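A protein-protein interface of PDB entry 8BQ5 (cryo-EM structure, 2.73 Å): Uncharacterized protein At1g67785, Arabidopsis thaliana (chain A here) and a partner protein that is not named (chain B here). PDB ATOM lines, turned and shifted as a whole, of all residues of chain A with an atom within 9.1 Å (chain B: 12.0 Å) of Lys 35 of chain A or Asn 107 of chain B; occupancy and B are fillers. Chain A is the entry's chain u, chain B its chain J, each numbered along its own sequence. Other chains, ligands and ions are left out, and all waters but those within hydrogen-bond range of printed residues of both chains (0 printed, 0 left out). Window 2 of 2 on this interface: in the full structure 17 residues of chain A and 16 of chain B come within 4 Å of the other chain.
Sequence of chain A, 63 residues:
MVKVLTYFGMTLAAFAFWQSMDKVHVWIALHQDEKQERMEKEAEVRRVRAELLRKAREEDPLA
The side-chain carboxylate (OD2) of Asp 106 of chain B lies within hydrogen-bond range of a ring nitrogen (ND1) of His 25 of chain A (3.5 Å). NZ of Lys 35 of chain A lies within hydrogen-bond range of OD1 of Asn 107 of chain B, 3.3 Å away.
Among the printed residues, merely in contact across the chains: His 25 of chain A with Phe 102 of chain B (3.99 Å), His 25 of chain A with Phe 103 of chain B (3.7 Å), Ile 28 of chain A with Phe 103 of chain B (3.7 Å), Ile 28 of chain A with Asp 106 of chain B (3.6 Å), Ala 29 of chain A with Pro 111 of chain B (3.6 Å), Gln 32 of chain A with Asn 107 of chain B (3.9 Å) and Gln 32 of chain A with Ile 110 of chain B (3.4 Å).
Lys 35 of chain A touches one residue of chain B. Asn 107 of chain B touches just these residues of chain A: Gln 32 and Lys 35. Of chain B, only Asn 107 and Ile 110 come within 4 Å of Gln 32 of chain A. No residue of chain B comes within 4 Å of Asp 33 of chain A. No residue of chain B comes within 4 Å of Gln 36 of chain A. No residue of chain B comes within 4 Å of Met 39 of chain A. Of the printed residues of chain A, Pro 111 of chain B touches Ala 29. Of the printed residues of chain A, Phe 102 of chain B touches His 25. Of the printed residues of chain B, Ile 28 of chain A touches Phe 103 and Asp 106. Of the printed residues of chain B, His 25 of chain A touches Phe 102 (3.99 Å), Phe 103 (3.7 Å) and Asp 106 (3.5 Å). Printed residues of chain A within 4 Å of Phe 103 of chain B: His 25 and Ile 28. Leu 105 of chain B touches none of the printed residues of chain A. Trp 99 of chain B touches none of the printed residues of chain A. The nearest residue of chain B that does not touch Lys 35 of chain A is Asp 106 of chain B (7.2 Å).
The side-chain amide oxygen (OE1) of Gln 32 of chain A lies close to the backbone carbonyl oxygen (O) of Ile 28 of chain A (3.4 Å).
Hydrophobic or aromatic side chains of chain A that line the printed part of chain B: His 25, Ile 28 and Ala 29. Among the printed residues, no Asp or Glu carboxylate lies within 4 Å of a Lys or Arg side-chain nitrogen of the other chain.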
ATOM      1  N   HIS A  25      26.076  -0.866 -18.312  1.00  0.00           N
ATOM      2  CA  HIS A  25      26.555  -2.200 -17.961  1.00  0.00           C
ATOM      3  C   HIS A  25      25.406  -3.107 -17.544  1.00  0.00           C
ATOM      4  O   HIS A  25      25.360  -4.284 -17.929  1.00  0.00           O
ATOM      5  CB  HIS A  25      27.597  -2.115 -16.848  1.00  0.00           C
ATOM      6  CG  HIS A  25      28.864  -1.436 -17.261  1.00  0.00           C
ATOM      7  ND1 HIS A  25      29.512  -1.725 -18.441  1.00  0.00           N
ATOM      8  CD2 HIS A  25      29.595  -0.471 -16.654  1.00  0.00           C
ATOM      9  CE1 HIS A  25      30.592  -0.970 -18.543  1.00  0.00           C
ATOM     10  NE2 HIS A  25      30.666  -0.201 -17.472  1.00  0.00           N
ATOM     11  N   ILE A  28      23.595  -4.171 -20.696  1.00  0.00           N
ATOM     12  CA  ILE A  28      24.340  -5.175 -21.451  1.00  0.00           C
ATOM     13  C   ILE A  28      24.242  -6.534 -20.771  1.00  0.00           C
ATOM     14  O   ILE A  28      24.144  -7.573 -21.436  1.00  0.00           O
ATOM     15  CB  ILE A  28      25.804  -4.733 -21.639  1.00  0.00           C
ATOM     16  CG1 ILE A  28      25.898  -3.657 -22.722  1.00  0.00           C
ATOM     17  CG2 ILE A  28      26.689  -5.918 -21.997  1.00  0.00           C
ATOM     18  CD1 ILE A  28      27.083  -2.740 -22.564  1.00  0.00           C
ATOM     19  N   ALA A  29      24.258  -6.550 -19.437  1.00  0.00           N
ATOM     20  CA  ALA A  29      24.097  -7.810 -18.718  1.00  0.00           C
ATOM     21  C   ALA A  29      22.716  -8.411 -18.953  1.00  0.00           C
ATOM     22  O   ALA A  29      22.576  -9.634 -19.069  1.00  0.00           O
ATOM     23  CB  ALA A  29      24.338  -7.601 -17.225  1.00  0.00           C
ATOM     24  N   LEU A  30      21.684  -7.567 -19.027  1.00  0.00           N
ATOM     25  CA  LEU A  30      20.320  -8.072 -19.163  1.00  0.00           C
ATOM     26  C   LEU A  30      20.060  -8.732 -20.513  1.00  0.00           C
ATOM     27  O   LEU A  30      19.095  -9.494 -20.636  1.00  0.00           O
ATOM     28  CB  LEU A  30      19.317  -6.939 -18.943  1.00  0.00           C
ATOM     29  CG  LEU A  30      18.956  -6.638 -17.486  1.00  0.00           C
ATOM     30  CD1 LEU A  30      18.292  -5.278 -17.365  1.00  0.00           C
ATOM     31  CD2 LEU A  30      18.061  -7.724 -16.914  1.00  0.00           C
ATOM     32  N   HIS A  31      20.889  -8.468 -21.522  1.00  0.00           N
ATOM     33  CA  HIS A  31      20.672  -8.981 -22.868  1.00  0.00           C
ATOM     34  C   HIS A  31      21.643 -10.096 -23.236  1.00  0.00           C
ATOM     35  O   HIS A  31      21.899 -10.320 -24.424  1.00  0.00           O
ATOM     36  CB  HIS A  31      20.756  -7.839 -23.878  1.00  0.00           C
ATOM     37  CG  HIS A  31      19.636  -6.855 -23.754  1.00  0.00           C
ATOM     38  ND1 HIS A  31      19.484  -6.043 -22.651  1.00  0.00           N
ATOM     39  CD2 HIS A  31      18.604  -6.566 -24.581  1.00  0.00           C
ATOM     40  CE1 HIS A  31      18.410  -5.290 -22.808  1.00  0.00           C
ATOM     41  NE2 HIS A  31      17.858  -5.588 -23.970  1.00  0.00           N
ATOM     42  N   GLN A  32      22.198 -10.791 -22.241  1.00  0.00           N
ATOM     43  CA  GLN A  32      23.072 -11.922 -22.524  1.00  0.00           C
ATOM     44  C   GLN A  32      22.291 -13.087 -23.118  1.00  0.00           C
ATOM     45  O   GLN A  32      22.757 -13.752 -24.046  1.00  0.00           O
ATOM     46  CB  GLN A  32      23.789 -12.367 -21.250  1.00  0.00           C
ATOM     47  CG  GLN A  32      24.976 -11.514 -20.841  1.00  0.00           C
ATOM     48  CD  GLN A  32      25.961 -11.305 -21.969  1.00  0.00           C
ATOM     49  OE1 GLN A  32      26.087 -10.204 -22.502  1.00  0.00           O
ATOM     50  NE2 GLN A  32      26.653 -12.370 -22.352  1.00  0.00           N
ATOM     51  N   ASP A  33      21.100 -13.355 -22.592  1.00  0.00           N
ATOM     52  CA  ASP A  33      20.342 -14.510 -23.057  1.00  0.00           C
ATOM     53  C   ASP A  33      19.905 -14.342 -24.506  1.00  0.00           C
ATOM     54  O   ASP A  33      20.009 -15.281 -25.304  1.00  0.00           O
ATOM     55  CB  ASP A  33      19.147 -14.728 -22.140  1.00  0.00           C
ATOM     56  CG  ASP A  33      19.549 -15.350 -20.825  1.00  0.00           C
ATOM     57  OD1 ASP A  33      19.102 -14.851 -19.772  1.00  0.00           O
ATOM     58  OD2 ASP A  33      20.324 -16.329 -20.846  1.00  0.00           O
ATOM     59  N   GLU A  34      19.431 -13.148 -24.869  1.00  0.00           N
ATOM     60  CA  GLU A  34      19.058 -12.886 -26.255  1.00  0.00           C
ATOM     61  C   GLU A  34      20.253 -13.053 -27.183  1.00  0.00           C
ATOM     62  O   GLU A  34      20.126 -13.612 -28.277  1.00  0.00           O
ATOM     63  CB  GLU A  34      18.485 -11.475 -26.386  1.00  0.00           C
ATOM     64  CG  GLU A  34      17.870 -10.924 -25.109  1.00  0.00           C
ATOM     65  CD  GLU A  34      16.536 -11.562 -24.777  1.00  0.00           C
ATOM     66  OE1 GLU A  34      16.331 -11.941 -23.604  1.00  0.00           O
ATOM     67  OE2 GLU A  34      15.690 -11.677 -25.688  1.00  0.00           O
ATOM     68  N   LYS A  35      21.422 -12.569 -26.762  1.00  0.00           N
ATOM     69  CA  LYS A  35      22.609 -12.659 -27.606  1.00  0.00           C
ATOM     70  C   LYS A  35      23.050 -14.107 -27.792  1.00  0.00           C
ATOM     71  O   LYS A  35      23.400 -14.514 -28.904  1.00  0.00           O
ATOM     72  CB  LYS A  35      23.736 -11.814 -27.014  1.00  0.00           C
ATOM     73  CG  LYS A  35      24.965 -11.713 -27.898  1.00  0.00           C
ATOM     74  CD  LYS A  35      25.666 -10.378 -27.716  1.00  0.00           C
ATOM     75  CE  LYS A  35      26.889 -10.513 -26.827  1.00  0.00           C
ATOM     76  NZ  LYS A  35      28.068  -9.805 -27.395  1.00  0.00           N
ATOM     77  N   GLN A  36      23.039 -14.902 -26.718  1.00  0.00           N
ATOM     78  CA  GLN A  36      23.371 -16.320 -26.857  1.00  0.00           C
ATOM     79  C   GLN A  36      22.352 -17.052 -27.723  1.00  0.00           C
ATOM     80  O   GLN A  36      22.719 -17.926 -28.514  1.00  0.00           O
ATOM     81  CB  GLN A  36      23.489 -16.985 -25.484  1.00  0.00           C
ATOM     82  CG  GLN A  36      23.974 -18.440 -25.484  1.00  0.00           C
ATOM     83  CD  GLN A  36      24.238 -19.012 -24.098  1.00  0.00           C
ATOM     84  OE1 GLN A  36      24.156 -18.319 -23.100  1.00  0.00           O
ATOM     85  NE2 GLN A  36      24.561 -20.292 -24.045  1.00  0.00           N
ATOM     86  N   GLU A  37      21.068 -16.722 -27.579  1.00  0.00           N
ATOM     87  CA  GLU A  37      20.043 -17.346 -28.412  1.00  0.00           C
ATOM     88  C   GLU A  37      20.249 -17.013 -29.885  1.00  0.00           C
ATOM     89  O   GLU A  37      20.143 -17.888 -30.755  1.00  0.00           O
ATOM     90  CB  GLU A  37      18.660 -16.894 -27.950  1.00  0.00           C
ATOM     91  CG  GLU A  37      17.505 -17.623 -28.603  1.00  0.00           C
ATOM     92  CD  GLU A  37      16.176 -16.952 -28.323  1.00  0.00           C
ATOM     93  OE1 GLU A  37      16.185 -15.823 -27.789  1.00  0.00           O
ATOM     94  OE2 GLU A  37      15.127 -17.553 -28.633  1.00  0.00           O
ATOM     95  N   ARG A  38      20.544 -15.746 -30.180  1.00  0.00           N
ATOM     96  CA  ARG A  38      20.821 -15.338 -31.552  1.00  0.00           C
ATOM     97  C   ARG A  38      22.066 -16.034 -32.087  1.00  0.00           C
ATOM     98  O   ARG A  38      22.092 -16.487 -33.240  1.00  0.00           O
ATOM     99  CB  ARG A  38      20.971 -13.818 -31.601  1.00  0.00           C
ATOM    100  CG  ARG A  38      21.239 -13.231 -32.971  1.00  0.00           C
ATOM    101  CD  ARG A  38      21.293 -11.714 -32.892  1.00  0.00           C
ATOM    102  NE  ARG A  38      21.527 -11.100 -34.197  1.00  0.00           N
ATOM    103  CZ  ARG A  38      21.433  -9.802 -34.452  1.00  0.00           C
ATOM    104  NH1 ARG A  38      21.087  -8.933 -33.517  1.00  0.00           N
ATOM    105  NH2 ARG A  38      21.687  -9.364 -35.684  1.00  0.00           N
ATOM    106  N   MET A  39      23.103 -16.145 -31.254  1.00  0.00           N
ATOM    107  CA  MET A  39      24.313 -16.854 -31.648  1.00  0.00           C
ATOM    108  C   MET A  39      24.019 -18.313 -31.968  1.00  0.00           C
ATOM    109  O   MET A  39      24.531 -18.856 -32.953  1.00  0.00           O
ATOM    110  CB  MET A  39      25.358 -16.753 -30.537  1.00  0.00           C
ATOM    111  CG  MET A  39      26.405 -15.673 -30.748  1.00  0.00           C
ATOM    112  SD  MET A  39      27.786 -16.277 -31.734  1.00  0.00           S
ATOM    113  CE  MET A  39      28.726 -17.164 -30.493  1.00  0.00           C
ATOM    114  N   GLU A  40      23.198 -18.964 -31.142  1.00  0.00           N
ATOM    115  CA  GLU A  40      22.848 -20.358 -31.392  1.00  0.00           C
ATOM    116  C   GLU A  40      22.066 -20.511 -32.687  1.00  0.00           C
ATOM    117  O   GLU A  40      22.322 -21.438 -33.463  1.00  0.00           O
ATOM    118  CB  GLU A  40      22.046 -20.925 -30.221  1.00  0.00           C
ATOM    119  CG  GLU A  40      22.863 -21.144 -28.970  1.00  0.00           C
ATOM    120  CD  GLU A  40      24.062 -22.036 -29.213  1.00  0.00           C
ATOM    121  OE1 GLU A  40      23.917 -23.056 -29.921  1.00  0.00           O
ATOM    122  OE2 GLU A  40      25.153 -21.710 -28.702  1.00  0.00           O
ATOM    123  N   LYS A  41      21.102 -19.622 -32.935  1.00  0.00           N
ATOM    124  CA  LYS A  41      20.323 -19.732 -34.165  1.00  0.00           C
ATOM    125  C   LYS A  41      21.212 -19.546 -35.389  1.00  0.00           C
ATOM    126  O   LYS A  41      21.097 -20.291 -36.370  1.00  0.00           O
ATOM    127  CB  LYS A  41      19.178 -18.720 -34.164  1.00  0.00           C
ATOM    128  CG  LYS A  41      18.452 -18.606 -35.498  1.00  0.00           C
ATOM    129  CD  LYS A  41      17.624 -17.332 -35.576  1.00  0.00           C
ATOM    130  CE  LYS A  41      18.211 -16.339 -36.562  1.00  0.00           C
ATOM    131  NZ  LYS A  41      17.412 -15.085 -36.639  1.00  0.00           N
ATOM    132  N   GLU A  42      22.130 -18.577 -35.339  1.00  0.00           N
ATOM    133  CA  GLU A  42      23.017 -18.349 -36.477  1.00  0.00           C
ATOM    134  C   GLU A  42      23.994 -19.508 -36.669  1.00  0.00           C
ATOM    135  O   GLU A  42      24.303 -19.886 -37.809  1.00  0.00           O
ATOM    136  CB  GLU A  42      23.755 -17.021 -36.294  1.00  0.00           C
ATOM    137  CG  GLU A  42      23.144 -15.842 -37.065  1.00  0.00           C
ATOM    138  CD  GLU A  42      21.723 -15.476 -36.636  1.00  0.00           C
ATOM    139  OE1 GLU A  42      21.137 -14.556 -37.248  1.00  0.00           O
ATOM    140  OE2 GLU A  42      21.187 -16.084 -35.688  1.00  0.00           O
ATOM    141  N   ALA A  43      24.490 -20.086 -35.572  1.00  0.00           N
ATOM    142  CA  ALA A  43      25.356 -21.255 -35.684  1.00  0.00           C
ATOM    143  C   ALA A  43      24.609 -22.430 -36.298  1.00  0.00           C
ATOM    144  O   ALA A  43      25.165 -23.169 -37.118  1.00  0.00           O
ATOM    145  CB  ALA A  43      25.915 -21.634 -34.313  1.00  0.00           C
ATOM    146  N   TRP B  98      36.220   3.582 -26.942  1.00  0.00           N
ATOM    147  CA  TRP B  98      35.261   3.413 -25.861  1.00  0.00           C
ATOM    148  C   TRP B  98      34.398   2.182 -26.075  1.00  0.00           C
ATOM    149  O   TRP B  98      34.343   1.293 -25.217  1.00  0.00           O
ATOM    150  CB  TRP B  98      34.397   4.669 -25.746  1.00  0.00           C
ATOM    151  CG  TRP B  98      33.223   4.516 -24.838  1.00  0.00           C
ATOM    152  CD1 TRP B  98      33.219   4.583 -23.477  1.00  0.00           C
ATOM    153  CD2 TRP B  98      31.871   4.264 -25.234  1.00  0.00           C
ATOM    154  NE1 TRP B  98      31.944   4.391 -22.999  1.00  0.00           N
ATOM    155  CE2 TRP B  98      31.099   4.192 -24.059  1.00  0.00           C
ATOM    156  CE3 TRP B  98      31.238   4.092 -26.468  1.00  0.00           C
ATOM    157  CZ2 TRP B  98      29.727   3.955 -24.084  1.00  0.00           C
ATOM    158  CZ3 TRP B  98      29.879   3.858 -26.490  1.00  0.00           C
ATOM    159  CH2 TRP B  98      29.137   3.793 -25.305  1.00  0.00           C
ATOM    160  N   TRP B  99      33.743   2.092 -27.234  1.00  0.00           N
ATOM    161  CA  TRP B  99      32.839   0.973 -27.465  1.00  0.00           C
ATOM    162  C   TRP B  99      33.594  -0.350 -27.513  1.00  0.00           C
ATOM    163  O   TRP B  99      33.118  -1.349 -26.961  1.00  0.00           O
ATOM    164  CB  TRP B  99      32.014   1.227 -28.735  1.00  0.00           C
ATOM    165  CG  TRP B  99      31.560   0.016 -29.531  1.00  0.00           C
ATOM    166  CD1 TRP B  99      31.176  -1.204 -29.048  1.00  0.00           C
ATOM    167  CD2 TRP B  99      31.342  -0.035 -30.947  1.00  0.00           C
ATOM    168  NE1 TRP B  99      30.799  -2.027 -30.077  1.00  0.00           N
ATOM    169  CE2 TRP B  99      30.881  -1.330 -31.254  1.00  0.00           C
ATOM    170  CE3 TRP B  99      31.511   0.883 -31.988  1.00  0.00           C
ATOM    171  CZ2 TRP B  99      30.590  -1.731 -32.555  1.00  0.00           C
ATOM    172  CZ3 TRP B  99      31.221   0.484 -33.277  1.00  0.00           C
ATOM    173  CH2 TRP B  99      30.768  -0.811 -33.551  1.00  0.00           C
ATOM    174  N   GLU B 100      34.775  -0.384 -28.125  1.00  0.00           N
ATOM    175  CA  GLU B 100      35.466  -1.662 -28.202  1.00  0.00           C
ATOM    176  C   GLU B 100      36.121  -2.056 -26.881  1.00  0.00           C
ATOM    177  O   GLU B 100      36.284  -3.251 -26.607  1.00  0.00           O
ATOM    178  CB  GLU B 100      36.512  -1.625 -29.320  1.00  0.00           C
ATOM    179  CG  GLU B 100      37.205  -2.952 -29.567  1.00  0.00           C
ATOM    180  CD  GLU B 100      36.316  -3.937 -30.308  1.00  0.00           C
ATOM    181  OE1 GLU B 100      35.719  -3.547 -31.332  1.00  0.00           O
ATOM    182  OE2 GLU B 100      36.214  -5.101 -29.865  1.00  0.00           O
ATOM    183  N   MET B 101      36.457  -1.088 -26.023  1.00  0.00           N
ATOM    184  CA  MET B 101      37.436  -1.328 -24.979  1.00  0.00           C
ATOM    185  C   MET B 101      36.912  -1.143 -23.559  1.00  0.00           C
ATOM    186  O   MET B 101      37.456  -1.763 -22.641  1.00  0.00           O
ATOM    187  CB  MET B 101      38.642  -0.406 -25.213  1.00  0.00           C
ATOM    188  CG  MET B 101      39.940  -0.944 -24.699  1.00  0.00           C
ATOM    189  SD  MET B 101      40.635  -2.291 -25.666  1.00  0.00           S
ATOM    190  CE  MET B 101      40.209  -1.771 -27.321  1.00  0.00           C
ATOM    191  N   PHE B 102      35.885  -0.314 -23.346  1.00  0.00           N
ATOM    192  CA  PHE B 102      35.236  -0.264 -22.039  1.00  0.00           C
ATOM    193  C   PHE B 102      34.316  -1.449 -21.788  1.00  0.00           C
ATOM    194  O   PHE B 102      33.919  -1.674 -20.639  1.00  0.00           O
ATOM    195  CB  PHE B 102      34.440   1.035 -21.870  1.00  0.00           C
ATOM    196  CG  PHE B 102      35.289   2.264 -21.723  1.00  0.00           C
ATOM    197  CD1 PHE B 102      35.313   2.954 -20.525  1.00  0.00           C
ATOM    198  CD2 PHE B 102      36.067   2.725 -22.765  1.00  0.00           C
ATOM    199  CE1 PHE B 102      36.087   4.085 -20.375  1.00  0.00           C
ATOM    200  CE2 PHE B 102      36.843   3.858 -22.623  1.00  0.00           C
ATOM    201  CZ  PHE B 102      36.854   4.537 -21.425  1.00  0.00           C
ATOM    202  N   PHE B 103      33.960  -2.204 -22.826  1.00  0.00           N
ATOM    203  CA  PHE B 103      33.117  -3.383 -22.676  1.00  0.00           C
ATOM    204  C   PHE B 103      33.841  -4.660 -23.082  1.00  0.00           C
ATOM    205  O   PHE B 103      33.195  -5.610 -23.542  1.00  0.00           O
ATOM    206  CB  PHE B 103      31.826  -3.214 -23.481  1.00  0.00           C
ATOM    207  CG  PHE B 103      31.224  -1.843 -23.363  1.00  0.00           C
ATOM    208  CD1 PHE B 103      30.568  -1.458 -22.206  1.00  0.00           C
ATOM    209  CD2 PHE B 103      31.332  -0.933 -24.399  1.00  0.00           C
ATOM    210  CE1 PHE B 103      30.023  -0.193 -22.089  1.00  0.00           C
ATOM    211  CE2 PHE B 103      30.790   0.331 -24.287  1.00  0.00           C
ATOM    212  CZ  PHE B 103      30.135   0.700 -23.129  1.00  0.00           C
ATOM    213  N   ILE B 104      35.163  -4.708 -22.916  1.00  0.00           N
ATOM    214  CA  ILE B 104      35.923  -5.880 -23.335  1.00  0.00           C
ATOM    215  C   ILE B 104      35.748  -7.019 -22.341  1.00  0.00           C
ATOM    216  O   ILE B 104      35.889  -8.193 -22.703  1.00  0.00           O
ATOM    217  CB  ILE B 104      37.400  -5.495 -23.527  1.00  0.00           C
ATOM    218  CG1 ILE B 104      38.181  -6.616 -24.201  1.00  0.00           C
ATOM    219  CG2 ILE B 104      38.032  -5.246 -22.196  1.00  0.00           C
ATOM    220  CD1 ILE B 104      39.643  -6.410 -24.166  1.00  0.00           C
ATOM    221  N   LEU B 105      35.431  -6.704 -21.086  1.00  0.00           N
ATOM    222  CA  LEU B 105      35.229  -7.734 -20.078  1.00  0.00           C
ATOM    223  C   LEU B 105      33.777  -8.178 -19.962  1.00  0.00           C
ATOM    224  O   LEU B 105      33.511  -9.173 -19.282  1.00  0.00           O
ATOM    225  CB  LEU B 105      35.720  -7.243 -18.711  1.00  0.00           C
ATOM    226  CG  LEU B 105      37.177  -6.792 -18.568  1.00  0.00           C
ATOM    227  CD1 LEU B 105      37.563  -6.694 -17.100  1.00  0.00           C
ATOM    228  CD2 LEU B 105      38.112  -7.738 -19.298  1.00  0.00           C
ATOM    229  N   ASP B 106      32.839  -7.486 -20.614  1.00  0.00           N
ATOM    230  CA  ASP B 106      31.424  -7.767 -20.388  1.00  0.00           C
ATOM    231  C   ASP B 106      31.046  -9.169 -20.853  1.00  0.00           C
ATOM    232  O   ASP B 106      30.311  -9.882 -20.159  1.00  0.00           O
ATOM    233  CB  ASP B 106      30.566  -6.711 -21.081  1.00  0.00           C
ATOM    234  CG  ASP B 106      30.658  -5.358 -20.403  1.00  0.00           C
ATOM    235  OD1 ASP B 106      31.781  -4.958 -20.036  1.00  0.00           O
ATOM    236  OD2 ASP B 106      29.613  -4.697 -20.234  1.00  0.00           O
ATOM    237  N   ASN B 107      31.538  -9.586 -22.019  1.00  0.00           N
ATOM    238  CA  ASN B 107      31.241 -10.929 -22.502  1.00  0.00           C
ATOM    239  C   ASN B 107      31.978 -11.999 -21.709  1.00  0.00           C
ATOM    240  O   ASN B 107      31.423 -13.077 -21.466  1.00  0.00           O
ATOM    241  CB  ASN B 107      31.586 -11.043 -23.987  1.00  0.00           C
ATOM    242  CG  ASN B 107      30.628 -10.268 -24.866  1.00  0.00           C
ATOM    243  OD1 ASN B 107      29.494  -9.992 -24.476  1.00  0.00           O
ATOM    244  ND2 ASN B 107      31.081  -9.908 -26.062  1.00  0.00           N
ATOM    245  N   GLU B 108      33.217 -11.726 -21.304  1.00  0.00           N
ATOM    246  CA  GLU B 108      33.976 -12.693 -20.520  1.00  0.00           C
ATOM    247  C   GLU B 108      33.585 -12.654 -19.048  1.00  0.00           C
ATOM    248  O   GLU B 108      33.447 -13.703 -18.412  1.00  0.00           O
ATOM    249  CB  GLU B 108      35.471 -12.431 -20.684  1.00  0.00           C
ATOM    250  CG  GLU B 108      36.365 -13.477 -20.057  1.00  0.00           C
ATOM    251  CD  GLU B 108      37.695 -13.596 -20.770  1.00  0.00           C
ATOM    252  OE1 GLU B 108      38.443 -14.553 -20.487  1.00  0.00           O
ATOM    253  OE2 GLU B 108      37.989 -12.728 -21.619  1.00  0.00           O
ATOM    254  N   SER B 109      33.398 -11.462 -18.496  1.00  0.00           N
ATOM    255  CA  SER B 109      33.042 -11.283 -17.090  1.00  0.00           C
ATOM    256  C   SER B 109      31.668 -10.623 -17.043  1.00  0.00           C
ATOM    257  O   SER B 109      31.549  -9.400 -16.951  1.00  0.00           O
ATOM    258  CB  SER B 109      34.090 -10.453 -16.366  1.00  0.00           C
ATOM    259  OG  SER B 109      35.158 -11.267 -15.920  1.00  0.00           O
ATOM    260  N   ILE B 110      30.632 -11.445 -17.106  1.00  0.00           N
ATOM    261  CA  ILE B 110      29.259 -10.943 -17.050  1.00  0.00           C
ATOM    262  C   ILE B 110      28.950 -10.520 -15.617  1.00  0.00           C
ATOM    263  O   ILE B 110      29.130 -11.325 -14.691  1.00  0.00           O
ATOM    264  CB  ILE B 110      28.287 -12.007 -17.538  1.00  0.00           C
ATOM    265  CG1 ILE B 110      28.693 -12.443 -18.943  1.00  0.00           C
ATOM    266  CG2 ILE B 110      26.862 -11.478 -17.547  1.00  0.00           C
ATOM    267  CD1 ILE B 110      27.946 -13.625 -19.441  1.00  0.00           C
ATOM    268  N   PRO B 111      28.513  -9.285 -15.394  1.00  0.00           N
ATOM    269  CA  PRO B 111      28.285  -8.820 -14.023  1.00  0.00           C
ATOM    270  C   PRO B 111      27.108  -9.520 -13.364  1.00  0.00           C
ATOM    271  O   PRO B 111      26.156  -9.952 -14.017  1.00  0.00           O
ATOM    272  CB  PRO B 111      28.010  -7.322 -14.198  1.00  0.00           C
ATOM    273  CG  PRO B 111      27.512  -7.192 -15.591  1.00  0.00           C
ATOM    274  CD  PRO B 111      28.217  -8.246 -16.393  1.00  0.00           C
ATOM    275  N   LEU B 112      27.188  -9.624 -12.042  1.00  0.00           N
ATOM    276  CA  LEU B 112      26.112 -10.180 -11.232  1.00  0.00           C
ATOM    277  C   LEU B 112      25.169  -9.045 -10.850  1.00  0.00           C
ATOM    278  O   LEU B 112      25.549  -8.138 -10.103  1.00  0.00           O
ATOM    279  CB  LEU B 112      26.678 -10.872  -9.995  1.00  0.00           C
ATOM    280  CG  LEU B 112      25.692 -11.551  -9.047  1.00  0.00           C
ATOM    281  CD1 LEU B 112      24.948 -12.667  -9.757  1.00  0.00           C
ATOM    282  CD2 LEU B 112      26.429 -12.083  -7.832  1.00  0.00           C
